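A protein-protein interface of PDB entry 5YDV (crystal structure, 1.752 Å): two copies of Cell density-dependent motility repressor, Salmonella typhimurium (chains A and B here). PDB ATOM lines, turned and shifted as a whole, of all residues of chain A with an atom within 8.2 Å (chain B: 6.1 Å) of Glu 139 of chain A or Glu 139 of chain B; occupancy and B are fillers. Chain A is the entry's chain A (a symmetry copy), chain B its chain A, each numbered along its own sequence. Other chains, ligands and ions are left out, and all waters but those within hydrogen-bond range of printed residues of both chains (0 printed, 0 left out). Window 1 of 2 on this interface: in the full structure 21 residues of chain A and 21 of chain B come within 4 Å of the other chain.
Glu 139 of chain B touches two residues of chain A.
Of the printed residues of chain A, Leu 140 of chain B touches Pro 24 (3.7 Å).
Of the printed residues of chain B, Met 137 of chain A touches Glu 139 (3.8 Å).
Printed residues of chain A within 4 Å of Gln 143 of chain B: Pro 24.
Printed residues of chain B within 4 Å of Pro 24 of chain A: Leu 140 (3.7 Å) and Gln 143 (3.8 Å).
The nearest residue of chain B that does not touch Glu 139 of chain A is Leu 20 of chain B (4.1 Å).
The nearest residue of chain A that does not touch Glu 139 of chain B is Leu 20 of chain A (4.1 Å).
The nearest printed residue of chain B that does not touch Ser 19 of chain A is Leu 140 of chain B (4.1 Å).
Of the 13 printed residues of chain B, 4 touch a printed residue of chain A.
Along chain B the printed residues that touch a printed residue of chain A span positions 137 to 143.
Of the 25 printed residues of chain A, 4 touch a printed residue of chain B.
Hydrophobic or aromatic side chains of chain A that line the printed part of chain B: Pro 24 and Met 137.
Among the printed residues, no Asp or Glu carboxylate lies within 4 Å of a Lys or Arg side-chain nitrogen of the other chain.
The backbone carbonyl oxygen of Ala 15 of chain A is in hydrogen-bond range of the side-chain hydroxyl of Ser 19 of chain A.
The side-chain hydroxyl (OG) of Ser 135 of chain A is in hydrogen-bond range of the backbone NH (N) of Met 137 of chain A, 3.0 Å away.
Among the printed residues, pairs that only touch across the chains: Pro 24 of chain A with Leu 140 of chain B (3.7 Å), Ser 19 of chain A with Met 137 of chain B (3.7 Å), Met 137 of chain A with Glu 139 of chain B (3.8 Å), Glu 139 of chain A with Met 137 of chain B (3.8 Å) and Pro 24 of chain A with Gln 143 of chain B (3.8 Å).
The side-chain carboxylate (OE1) of Glu 139 of chain A sits close to the side-chain carboxylate (OE1) of Glu 139 of chain B (2.7 Å).
Met 137 of chain A touches Glu 139 of chain B, and with the chains exchanged Glu 139 of chain A touches Met 137 of chain B.
Glu 139 of chain B touches its own counterpart, Glu 139 of chain A.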
ATOM      1  N   ALA A  15     -24.597  18.901 -23.191  1.00  0.00           N
ATOM      2  CA  ALA A  15     -23.747  19.823 -23.928  1.00  0.00           C
ATOM      3  C   ALA A  15     -22.417  19.149 -24.237  1.00  0.00           C
ATOM      4  O   ALA A  15     -21.924  18.326 -23.461  1.00  0.00           O
ATOM      5  CB  ALA A  15     -23.521  21.106 -23.131  1.00  0.00           C
ATOM      6  N   HIS A  16     -21.846  19.502 -25.394  1.00  0.00           N
ATOM      7  CA  HIS A  16     -20.655  18.816 -25.902  1.00  0.00           C
ATOM      8  C   HIS A  16     -19.538  18.740 -24.865  1.00  0.00           C
ATOM      9  O   HIS A  16     -18.867  17.709 -24.739  1.00  0.00           O
ATOM     10  CB  HIS A  16     -20.141  19.518 -27.162  1.00  0.00           C
ATOM     11  CG  HIS A  16     -21.072  19.436 -28.333  1.00  0.00           C
ATOM     12  ND1 HIS A  16     -21.296  18.265 -29.023  1.00  0.00           N
ATOM     13  CD2 HIS A  16     -21.819  20.384 -28.945  1.00  0.00           C
ATOM     14  CE1 HIS A  16     -22.153  18.491 -30.004  1.00  0.00           C
ATOM     15  NE2 HIS A  16     -22.486  19.768 -29.978  1.00  0.00           N
ATOM     16  N   SER A  17     -19.334  19.817 -24.099  1.00  0.00           N
ATOM     17  CA  SER A  17     -18.124  19.953 -23.294  1.00  0.00           C
ATOM     18  C   SER A  17     -18.144  19.139 -22.006  1.00  0.00           C
ATOM     19  O   SER A  17     -17.070  18.803 -21.494  1.00  0.00           O
ATOM     20  CB  SER A  17     -17.872  21.424 -22.962  1.00  0.00           C
ATOM     21  OG  SER A  17     -18.163  22.252 -24.076  1.00  0.00           O
ATOM     22  N   LEU A  18     -19.314  18.817 -21.461  1.00  0.00           N
ATOM     23  CA  LEU A  18     -19.368  18.023 -20.243  1.00  0.00           C
ATOM     24  C   LEU A  18     -19.799  16.586 -20.492  1.00  0.00           C
ATOM     25  O   LEU A  18     -19.926  15.821 -19.535  1.00  0.00           O
ATOM     26  CB  LEU A  18     -20.290  18.686 -19.202  1.00  0.00           C
ATOM     27  CG  LEU A  18     -21.737  19.035 -19.551  1.00  0.00           C
ATOM     28  CD1 LEU A  18     -22.616  17.814 -19.577  1.00  0.00           C
ATOM     29  CD2 LEU A  18     -22.288  20.049 -18.552  1.00  0.00           C
ATOM     30  N   SER A  19     -20.032  16.200 -21.748  1.00  0.00           N
ATOM     31  CA  SER A  19     -20.470  14.836 -22.032  1.00  0.00           C
ATOM     32  C   SER A  19     -19.421  13.820 -21.599  1.00  0.00           C
ATOM     33  O   SER A  19     -19.737  12.828 -20.933  1.00  0.00           O
ATOM     34  CB  SER A  19     -20.786  14.681 -23.521  1.00  0.00           C
ATOM     35  OG  SER A  19     -21.856  15.521 -23.912  1.00  0.00           O
ATOM     36  N   LEU A  20     -18.157  14.064 -21.955  1.00  0.00           N
ATOM     37  CA  LEU A  20     -17.100  13.100 -21.661  1.00  0.00           C
ATOM     38  C   LEU A  20     -16.774  13.054 -20.174  1.00  0.00           C
ATOM     39  O   LEU A  20     -16.576  11.975 -19.610  1.00  0.00           O
ATOM     40  CB  LEU A  20     -15.841  13.431 -22.461  1.00  0.00           C
ATOM     41  CG  LEU A  20     -14.654  12.472 -22.269  1.00  0.00           C
ATOM     42  CD1 LEU A  20     -15.083  11.007 -22.206  1.00  0.00           C
ATOM     43  CD2 LEU A  20     -13.587  12.677 -23.331  1.00  0.00           C
ATOM     44  N   GLY A  21     -16.660  14.217 -19.530  1.00  0.00           N
ATOM     45  CA  GLY A  21     -16.295  14.222 -18.123  1.00  0.00           C
ATOM     46  C   GLY A  21     -17.408  13.724 -17.220  1.00  0.00           C
ATOM     47  O   GLY A  21     -17.162  12.972 -16.272  1.00  0.00           O
ATOM     48  N   PRO A  24     -19.553   9.288 -17.798  1.00  0.00           N
ATOM     49  CA  PRO A  24     -19.007   8.048 -17.220  1.00  0.00           C
ATOM     50  C   PRO A  24     -19.114   7.982 -15.710  1.00  0.00           C
ATOM     51  O   PRO A  24     -19.327   6.889 -15.167  1.00  0.00           O
ATOM     52  CB  PRO A  24     -17.543   8.060 -17.684  1.00  0.00           C
ATOM     53  CG  PRO A  24     -17.566   8.869 -18.932  1.00  0.00           C
ATOM     54  CD  PRO A  24     -18.578   9.942 -18.687  1.00  0.00           C
ATOM     55  N   TYR A 107     -13.855  27.565 -28.774  1.00  0.00           N
ATOM     56  CA  TYR A 107     -15.133  26.926 -29.042  1.00  0.00           C
ATOM     57  C   TYR A 107     -15.909  27.733 -30.081  1.00  0.00           C
ATOM     58  O   TYR A 107     -15.583  28.882 -30.385  1.00  0.00           O
ATOM     59  CB  TYR A 107     -15.958  26.800 -27.753  1.00  0.00           C
ATOM     60  CG  TYR A 107     -15.245  26.066 -26.639  1.00  0.00           C
ATOM     61  CD1 TYR A 107     -14.327  26.721 -25.827  1.00  0.00           C
ATOM     62  CD2 TYR A 107     -15.480  24.719 -26.410  1.00  0.00           C
ATOM     63  CE1 TYR A 107     -13.658  26.055 -24.826  1.00  0.00           C
ATOM     64  CE2 TYR A 107     -14.829  24.043 -25.396  1.00  0.00           C
ATOM     65  CZ  TYR A 107     -13.917  24.719 -24.606  1.00  0.00           C
ATOM     66  OH  TYR A 107     -13.260  24.059 -23.594  1.00  0.00           O
ATOM     67  N   PHE A 133      -8.170  27.838 -34.787  1.00  0.00           N
ATOM     68  CA  PHE A 133      -8.879  26.563 -34.790  1.00  0.00           C
ATOM     69  C   PHE A 133     -10.138  26.742 -33.960  1.00  0.00           C
ATOM     70  O   PHE A 133     -10.028  27.147 -32.802  1.00  0.00           O
ATOM     71  CB  PHE A 133      -7.995  25.447 -34.189  1.00  0.00           C
ATOM     72  CG  PHE A 133      -8.541  24.058 -34.371  1.00  0.00           C
ATOM     73  CD1 PHE A 133      -8.115  23.274 -35.433  1.00  0.00           C
ATOM     74  CD2 PHE A 133      -9.463  23.531 -33.485  1.00  0.00           C
ATOM     75  CE1 PHE A 133      -8.617  21.998 -35.620  1.00  0.00           C
ATOM     76  CE2 PHE A 133      -9.972  22.250 -33.664  1.00  0.00           C
ATOM     77  CZ  PHE A 133      -9.539  21.482 -34.735  1.00  0.00           C
ATOM     78  N   SER A 135     -13.767  24.696 -32.762  1.00  0.00           N
ATOM     79  CA  SER A 135     -14.443  23.413 -32.684  1.00  0.00           C
ATOM     80  C   SER A 135     -15.274  23.394 -31.416  1.00  0.00           C
ATOM     81  O   SER A 135     -14.877  23.956 -30.394  1.00  0.00           O
ATOM     82  CB  SER A 135     -13.439  22.251 -32.685  1.00  0.00           C
ATOM     83  OG  SER A 135     -14.039  21.053 -32.220  1.00  0.00           O
ATOM     84  N   SER A 136     -16.419  22.719 -31.489  1.00  0.00           N
ATOM     85  CA  SER A 136     -17.250  22.524 -30.308  1.00  0.00           C
ATOM     86  C   SER A 136     -16.678  21.485 -29.350  1.00  0.00           C
ATOM     87  O   SER A 136     -17.051  21.483 -28.172  1.00  0.00           O
ATOM     88  CB  SER A 136     -18.658  22.104 -30.733  1.00  0.00           C
ATOM     89  OG  SER A 136     -18.607  21.107 -31.744  1.00  0.00           O
ATOM     90  N   MET A 137     -15.777  20.618 -29.815  1.00  0.00           N
ATOM     91  CA  MET A 137     -15.335  19.456 -29.046  1.00  0.00           C
ATOM     92  C   MET A 137     -14.194  19.847 -28.114  1.00  0.00           C
ATOM     93  O   MET A 137     -13.078  20.128 -28.566  1.00  0.00           O
ATOM     94  CB  MET A 137     -14.911  18.324 -29.978  1.00  0.00           C
ATOM     95  CG  MET A 137     -14.621  17.015 -29.253  1.00  0.00           C
ATOM     96  SD  MET A 137     -14.163  15.676 -30.372  1.00  0.00           S
ATOM     97  CE  MET A 137     -15.459  15.819 -31.605  1.00  0.00           C
ATOM     98  N   SER A 138     -14.477  19.829 -26.808  1.00  0.00           N
ATOM     99  CA  SER A 138     -13.476  20.123 -25.784  1.00  0.00           C
ATOM    100  C   SER A 138     -12.224  19.271 -25.941  1.00  0.00           C
ATOM    101  O   SER A 138     -11.102  19.762 -25.772  1.00  0.00           O
ATOM    102  CB  SER A 138     -14.078  19.899 -24.392  1.00  0.00           C
ATOM    103  OG  SER A 138     -14.744  21.051 -23.913  1.00  0.00           O
ATOM    104  N   GLU A 139     -12.397  17.987 -26.259  1.00  0.00           N
ATOM    105  CA  GLU A 139     -11.263  17.070 -26.307  1.00  0.00           C
ATOM    106  C   GLU A 139     -10.397  17.307 -27.533  1.00  0.00           C
ATOM    107  O   GLU A 139      -9.188  17.065 -27.491  1.00  0.00           O
ATOM    108  CB  GLU A 139     -11.755  15.624 -26.284  1.00  0.00           C
ATOM    109  CG  GLU A 139     -12.940  15.401 -25.364  1.00  0.00           C
ATOM    110  CD  GLU A 139     -14.272  15.552 -26.075  1.00  0.00           C
ATOM    111  OE1 GLU A 139     -14.720  14.579 -26.717  1.00  0.00           O
ATOM    112  OE2 GLU A 139     -14.872  16.645 -25.992  1.00  0.00           O
ATOM    113  N   LEU A 140     -11.002  17.764 -28.626  1.00  0.00           N
ATOM    114  CA  LEU A 140     -10.230  18.165 -29.796  1.00  0.00           C
ATOM    115  C   LEU A 140      -9.426  19.429 -29.508  1.00  0.00           C
ATOM    116  O   LEU A 140      -8.237  19.507 -29.843  1.00  0.00           O
ATOM    117  CB  LEU A 140     -11.173  18.364 -30.986  1.00  0.00           C
ATOM    118  CG  LEU A 140     -10.613  18.712 -32.361  1.00  0.00           C
ATOM    119  CD1 LEU A 140      -9.429  17.832 -32.692  1.00  0.00           C
ATOM    120  CD2 LEU A 140     -11.715  18.552 -33.414  1.00  0.00           C
ATOM    121  N   LEU A 141     -10.056  20.434 -28.891  1.00  0.00           N
ATOM    122  CA  LEU A 141      -9.323  21.643 -28.520  1.00  0.00           C
ATOM    123  C   LEU A 141      -8.160  21.309 -27.598  1.00  0.00           C
ATOM    124  O   LEU A 141      -7.065  21.868 -27.733  1.00  0.00           O
ATOM    125  CB  LEU A 141     -10.250  22.653 -27.837  1.00  0.00           C
ATOM    126  CG  LEU A 141     -11.294  23.369 -28.694  1.00  0.00           C
ATOM    127  CD1 LEU A 141     -11.967  24.465 -27.870  1.00  0.00           C
ATOM    128  CD2 LEU A 141     -10.659  23.943 -29.952  1.00  0.00           C
ATOM    129  N   LYS A 142      -8.390  20.417 -26.634  1.00  0.00           N
ATOM    130  CA  LYS A 142      -7.327  20.043 -25.710  1.00  0.00           C
ATOM    131  C   LYS A 142      -6.156  19.405 -26.451  1.00  0.00           C
ATOM    132  O   LYS A 142      -4.997  19.751 -26.200  1.00  0.00           O
ATOM    133  CB  LYS A 142      -7.893  19.116 -24.627  1.00  0.00           C
ATOM    134  CG  LYS A 142      -6.864  18.513 -23.693  1.00  0.00           C
ATOM    135  CD  LYS A 142      -7.551  17.695 -22.611  1.00  0.00           C
ATOM    136  CE  LYS A 142      -6.692  16.539 -22.153  1.00  0.00           C
ATOM    137  NZ  LYS A 142      -7.431  15.658 -21.205  1.00  0.00           N
ATOM    138  N   GLN A 143      -6.434  18.507 -27.405  1.00  0.00           N
ATOM    139  CA  GLN A 143      -5.339  17.850 -28.121  1.00  0.00           C
ATOM    140  C   GLN A 143      -4.573  18.830 -29.006  1.00  0.00           C
ATOM    141  O   GLN A 143      -3.341  18.753 -29.114  1.00  0.00           O
ATOM    142  CB  GLN A 143      -5.870  16.694 -28.965  1.00  0.00           C
ATOM    143  CG  GLN A 143      -4.757  15.837 -29.573  1.00  0.00           C
ATOM    144  CD  GLN A 143      -3.956  15.102 -28.510  1.00  0.00           C
ATOM    145  OE1 GLN A 143      -2.726  15.193 -28.465  1.00  0.00           O
ATOM    146  NE2 GLN A 143      -4.657  14.379 -27.641  1.00  0.00           N
ATOM    147  N   VAL A 144      -5.282  19.742 -29.672  1.00  0.00           N
ATOM    148  CA  VAL A 144      -4.610  20.736 -30.501  1.00  0.00           C
ATOM    149  C   VAL A 144      -3.755  21.660 -29.635  1.00  0.00           C
ATOM    150  O   VAL A 144      -2.651  22.058 -30.022  1.00  0.00           O
ATOM    151  CB  VAL A 144      -5.655  21.506 -31.335  1.00  0.00           C
ATOM    152  CG1 VAL A 144      -5.007  22.592 -32.157  1.00  0.00           C
ATOM    153  CG2 VAL A 144      -6.377  20.538 -32.249  1.00  0.00           C
ATOM    154  N   ALA A 145      -4.233  21.987 -28.432  1.00  0.00           N
ATOM    155  CA  ALA A 145      -3.414  22.778 -27.522  1.00  0.00           C
ATOM    156  C   ALA A 145      -2.200  21.985 -27.063  1.00  0.00           C
ATOM    157  O   ALA A 145      -1.084  22.517 -27.002  1.00  0.00           O
ATOM    158  CB  ALA A 145      -4.247  23.231 -26.328  1.00  0.00           C
ATOM    159  N   MET A 146      -2.391  20.701 -26.767  1.00  0.00           N
ATOM    160  CA  MET A 146      -1.261  19.897 -26.324  1.00  0.00           C
ATOM    161  C   MET A 146      -0.221  19.768 -27.428  1.00  0.00           C
ATOM    162  O   MET A 146       0.981  19.738 -27.150  1.00  0.00           O
ATOM    163  CB  MET A 146      -1.755  18.532 -25.859  1.00  0.00           C
ATOM    164  CG  MET A 146      -2.536  18.600 -24.559  1.00  0.00           C
ATOM    165  SD  MET A 146      -2.903  16.979 -23.880  1.00  0.00           S
ATOM    166  CE  MET A 146      -4.078  16.345 -25.067  1.00  0.00           C
ATOM    167  N   LEU A 154      -9.667  26.074 -21.197  1.00  0.00           N
ATOM    168  CA  LEU A 154     -10.201  24.739 -20.956  1.00  0.00           C
ATOM    169  C   LEU A 154     -10.591  24.564 -19.495  1.00  0.00           C
ATOM    170  O   LEU A 154      -9.973  25.158 -18.602  1.00  0.00           O
ATOM    171  CB  LEU A 154      -9.182  23.656 -21.338  1.00  0.00           C
ATOM    172  CG  LEU A 154      -8.855  23.544 -22.832  1.00  0.00           C
ATOM    173  CD1 LEU A 154      -7.657  22.647 -23.018  1.00  0.00           C
ATOM    174  CD2 LEU A 154     -10.046  22.984 -23.572  1.00  0.00           C
ATOM    175  N   PRO A 155     -11.593  23.727 -19.228  1.00  0.00           N
ATOM    176  CA  PRO A 155     -12.049  23.537 -17.846  1.00  0.00           C
ATOM    177  C   PRO A 155     -11.067  22.706 -17.042  1.00  0.00           C
ATOM    178  O   PRO A 155     -10.396  21.806 -17.562  1.00  0.00           O
ATOM    179  CB  PRO A 155     -13.387  22.808 -18.012  1.00  0.00           C
ATOM    180  CG  PRO A 155     -13.248  22.079 -19.334  1.00  0.00           C
ATOM    181  CD  PRO A 155     -12.393  22.961 -20.201  1.00  0.00           C
ATOM    182  N   ALA A 158     -10.801  18.804 -17.187  1.00  0.00           N
ATOM    183  CA  ALA A 158     -10.310  18.175 -18.407  1.00  0.00           C
ATOM    184  C   ALA A 158      -8.793  18.218 -18.528  1.00  0.00           C
ATOM    185  O   ALA A 158      -8.216  17.382 -19.235  1.00  0.00           O
ATOM    186  CB  ALA A 158     -10.946  18.844 -19.627  1.00  0.00           C
ATOM    187  N   HIS B  16     -18.617  12.198 -36.220  1.00  0.00           N
ATOM    188  CA  HIS B  16     -18.248  12.225 -34.803  1.00  0.00           C
ATOM    189  C   HIS B  16     -17.056  11.324 -34.493  1.00  0.00           C
ATOM    190  O   HIS B  16     -16.173  11.699 -33.712  1.00  0.00           O
ATOM    191  CB  HIS B  16     -19.444  11.811 -33.940  1.00  0.00           C
ATOM    192  CG  HIS B  16     -20.592  12.771 -33.983  1.00  0.00           C
ATOM    193  ND1 HIS B  16     -20.542  14.017 -33.394  1.00  0.00           N
ATOM    194  CD2 HIS B  16     -21.827  12.661 -34.527  1.00  0.00           C
ATOM    195  CE1 HIS B  16     -21.692  14.639 -33.584  1.00  0.00           C
ATOM    196  NE2 HIS B  16     -22.489  13.839 -34.270  1.00  0.00           N
ATOM    197  N   SER B  17     -17.002  10.138 -35.108  1.00  0.00           N
ATOM    198  CA  SER B  17     -16.077   9.100 -34.667  1.00  0.00           C
ATOM    199  C   SER B  17     -14.640   9.315 -35.129  1.00  0.00           C
ATOM    200  O   SER B  17     -13.721   8.808 -34.477  1.00  0.00           O
ATOM    201  CB  SER B  17     -16.560   7.726 -35.135  1.00  0.00           C
ATOM    202  OG  SER B  17     -17.969   7.617 -35.012  1.00  0.00           O
ATOM    203  N   LEU B  20     -11.781  13.187 -33.519  1.00  0.00           N
ATOM    204  CA  LEU B  20     -10.684  13.240 -32.556  1.00  0.00           C
ATOM    205  C   LEU B  20      -9.413  12.611 -33.112  1.00  0.00           C
ATOM    206  O   LEU B  20      -8.316  13.143 -32.921  1.00  0.00           O
ATOM    207  CB  LEU B  20     -11.084  12.546 -31.255  1.00  0.00           C
ATOM    208  CG  LEU B  20     -10.027  12.556 -30.138  1.00  0.00           C
ATOM    209  CD1 LEU B  20      -9.299  13.895 -30.027  1.00  0.00           C
ATOM    210  CD2 LEU B  20     -10.619  12.151 -28.799  1.00  0.00           C
ATOM    211  N   SER B 136     -23.371   8.696 -29.733  1.00  0.00           N
ATOM    212  CA  SER B 136     -22.618   8.925 -30.959  1.00  0.00           C
ATOM    213  C   SER B 136     -21.123   9.089 -30.712  1.00  0.00           C
ATOM    214  O   SER B 136     -20.335   8.917 -31.647  1.00  0.00           O
ATOM    215  CB  SER B 136     -23.157  10.167 -31.671  1.00  0.00           C
ATOM    216  OG  SER B 136     -23.362  11.230 -30.749  1.00  0.00           O
ATOM    217  N   MET B 137     -20.713   9.403 -29.481  1.00  0.00           N
ATOM    218  CA  MET B 137     -19.336   9.795 -29.189  1.00  0.00           C
ATOM    219  C   MET B 137     -18.476   8.559 -28.955  1.00  0.00           C
ATOM    220  O   MET B 137     -18.626   7.869 -27.939  1.00  0.00           O
ATOM    221  CB  MET B 137     -19.286  10.728 -27.982  1.00  0.00           C
ATOM    222  CG  MET B 137     -17.910  11.331 -27.734  1.00  0.00           C
ATOM    223  SD  MET B 137     -17.879  12.464 -26.330  1.00  0.00           S
ATOM    224  CE  MET B 137     -19.316  13.476 -26.691  1.00  0.00           C
ATOM    225  N   SER B 138     -17.552   8.306 -29.886  1.00  0.00           N
ATOM    226  CA  SER B 138     -16.613   7.191 -29.778  1.00  0.00           C
ATOM    227  C   SER B 138     -15.862   7.197 -28.452  1.00  0.00           C
ATOM    228  O   SER B 138     -15.650   6.142 -27.844  1.00  0.00           O
ATOM    229  CB  SER B 138     -15.610   7.246 -30.936  1.00  0.00           C
ATOM    230  OG  SER B 138     -16.093   6.580 -32.086  1.00  0.00           O
ATOM    231  N   GLU B 139     -15.446   8.379 -27.993  1.00  0.00           N
ATOM    232  CA  GLU B 139     -14.614   8.464 -26.799  1.00  0.00           C
ATOM    233  C   GLU B 139     -15.414   8.199 -25.534  1.00  0.00           C
ATOM    234  O   GLU B 139     -14.864   7.698 -24.549  1.00  0.00           O
ATOM    235  CB  GLU B 139     -13.947   9.836 -26.719  1.00  0.00           C
ATOM    236  CG  GLU B 139     -13.492  10.368 -28.065  1.00  0.00           C
ATOM    237  CD  GLU B 139     -14.544  11.224 -28.744  1.00  0.00           C
ATOM    238  OE1 GLU B 139     -14.637  12.426 -28.419  1.00  0.00           O
ATOM    239  OE2 GLU B 139     -15.278  10.696 -29.606  1.00  0.00           O
ATOM    240  N   LEU B 140     -16.699   8.541 -25.543  1.00  0.00           N
ATOM    241  CA  LEU B 140     -17.576   8.185 -24.435  1.00  0.00           C
ATOM    242  C   LEU B 140     -17.805   6.677 -24.386  1.00  0.00           C
ATOM    243  O   LEU B 140     -17.728   6.065 -23.314  1.00  0.00           O
ATOM    244  CB  LEU B 140     -18.900   8.943 -24.567  1.00  0.00           C
ATOM    245  CG  LEU B 140     -19.972   8.813 -23.491  1.00  0.00           C
ATOM    246  CD1 LEU B 140     -19.362   8.934 -22.113  1.00  0.00           C
ATOM    247  CD2 LEU B 140     -21.041   9.890 -23.705  1.00  0.00           C
ATOM    248  N   LEU B 141     -18.089   6.059 -25.537  1.00  0.00           N
ATOM    249  CA  LEU B 141     -18.245   4.606 -25.571  1.00  0.00           C
ATOM    250  C   LEU B 141     -16.983   3.915 -25.079  1.00  0.00           C
ATOM    251  O   LEU B 141     -17.051   2.922 -24.345  1.00  0.00           O
ATOM    252  CB  LEU B 141     -18.576   4.128 -26.988  1.00  0.00           C
ATOM    253  CG  LEU B 141     -19.963   4.440 -27.550  1.00  0.00           C
ATOM    254  CD1 LEU B 141     -20.154   3.709 -28.877  1.00  0.00           C
ATOM    255  CD2 LEU B 141     -21.049   4.056 -26.554  1.00  0.00           C
ATOM    256  N   LYS B 142     -15.819   4.412 -25.498  1.00  0.00           N
ATOM    257  CA  LYS B 142     -14.564   3.806 -25.070  1.00  0.00           C
ATOM    258  C   LYS B 142     -14.408   3.883 -23.554  1.00  0.00           C
ATOM    259  O   LYS B 142     -14.040   2.892 -22.915  1.00  0.00           O
ATOM    260  CB  LYS B 142     -13.396   4.479 -25.801  1.00  0.00           C
ATOM    261  CG  LYS B 142     -12.017   4.064 -25.330  1.00  0.00           C
ATOM    262  CD  LYS B 142     -10.948   4.720 -26.189  1.00  0.00           C
ATOM    263  CE  LYS B 142      -9.681   4.978 -25.407  1.00  0.00           C
ATOM    264  NZ  LYS B 142      -8.697   5.755 -26.212  1.00  0.00           N
ATOM    265  N   GLN B 143     -14.729   5.034 -22.950  1.00  0.00           N
ATOM    266  CA  GLN B 143     -14.567   5.160 -21.500  1.00  0.00           C
ATOM    267  C   GLN B 143     -15.550   4.271 -20.741  1.00  0.00           C
ATOM    268  O   GLN B 143     -15.199   3.680 -19.711  1.00  0.00           O
ATOM    269  CB  GLN B 143     -14.740   6.613 -21.067  1.00  0.00           C
ATOM    270  CG  GLN B 143     -14.377   6.847 -19.598  1.00  0.00           C
ATOM    271  CD  GLN B 143     -12.898   6.618 -19.330  1.00  0.00           C
ATOM    272  OE1 GLN B 143     -12.525   5.849 -18.440  1.00  0.00           O
ATOM    273  NE2 GLN B 143     -12.050   7.279 -20.114  1.00  0.00           N
ATOM    274  N   VAL B 144     -16.793   4.184 -21.215  1.00  0.00           N
ATOM    275  CA  VAL B 144     -17.770   3.320 -20.564  1.00  0.00           C
ATOM    276  C   VAL B 144     -17.348   1.856 -20.684  1.00  0.00           C
ATOM    277  O   VAL B 144     -17.517   1.063 -19.752  1.00  0.00           O
ATOM    278  CB  VAL B 144     -19.170   3.584 -21.156  1.00  0.00           C
ATOM    279  CG1 VAL B 144     -20.201   2.659 -20.558  1.00  0.00           C
ATOM    280  CG2 VAL B 144     -19.562   5.022 -20.892  1.00  0.00           C
ATOM    281  N   MET B 146     -14.180   0.899 -20.908  1.00  0.00           N
ATOM    282  CA  MET B 146     -13.035   0.741 -20.023  1.00  0.00           C
ATOM    283  C   MET B 146     -13.482   0.619 -18.573  1.00  0.00           C
ATOM    284  O   MET B 146     -12.870  -0.116 -17.794  1.00  0.00           O
ATOM    285  CB  MET B 146     -12.074   1.909 -20.217  1.00  0.00           C
ATOM    286  CG  MET B 146     -11.360   1.869 -21.556  1.00  0.00           C
ATOM    287  SD  MET B 146     -10.053   3.093 -21.687  1.00  0.00           S
ATOM    288  CE  MET B 146     -10.984   4.617 -21.728  1.00  0.00           C
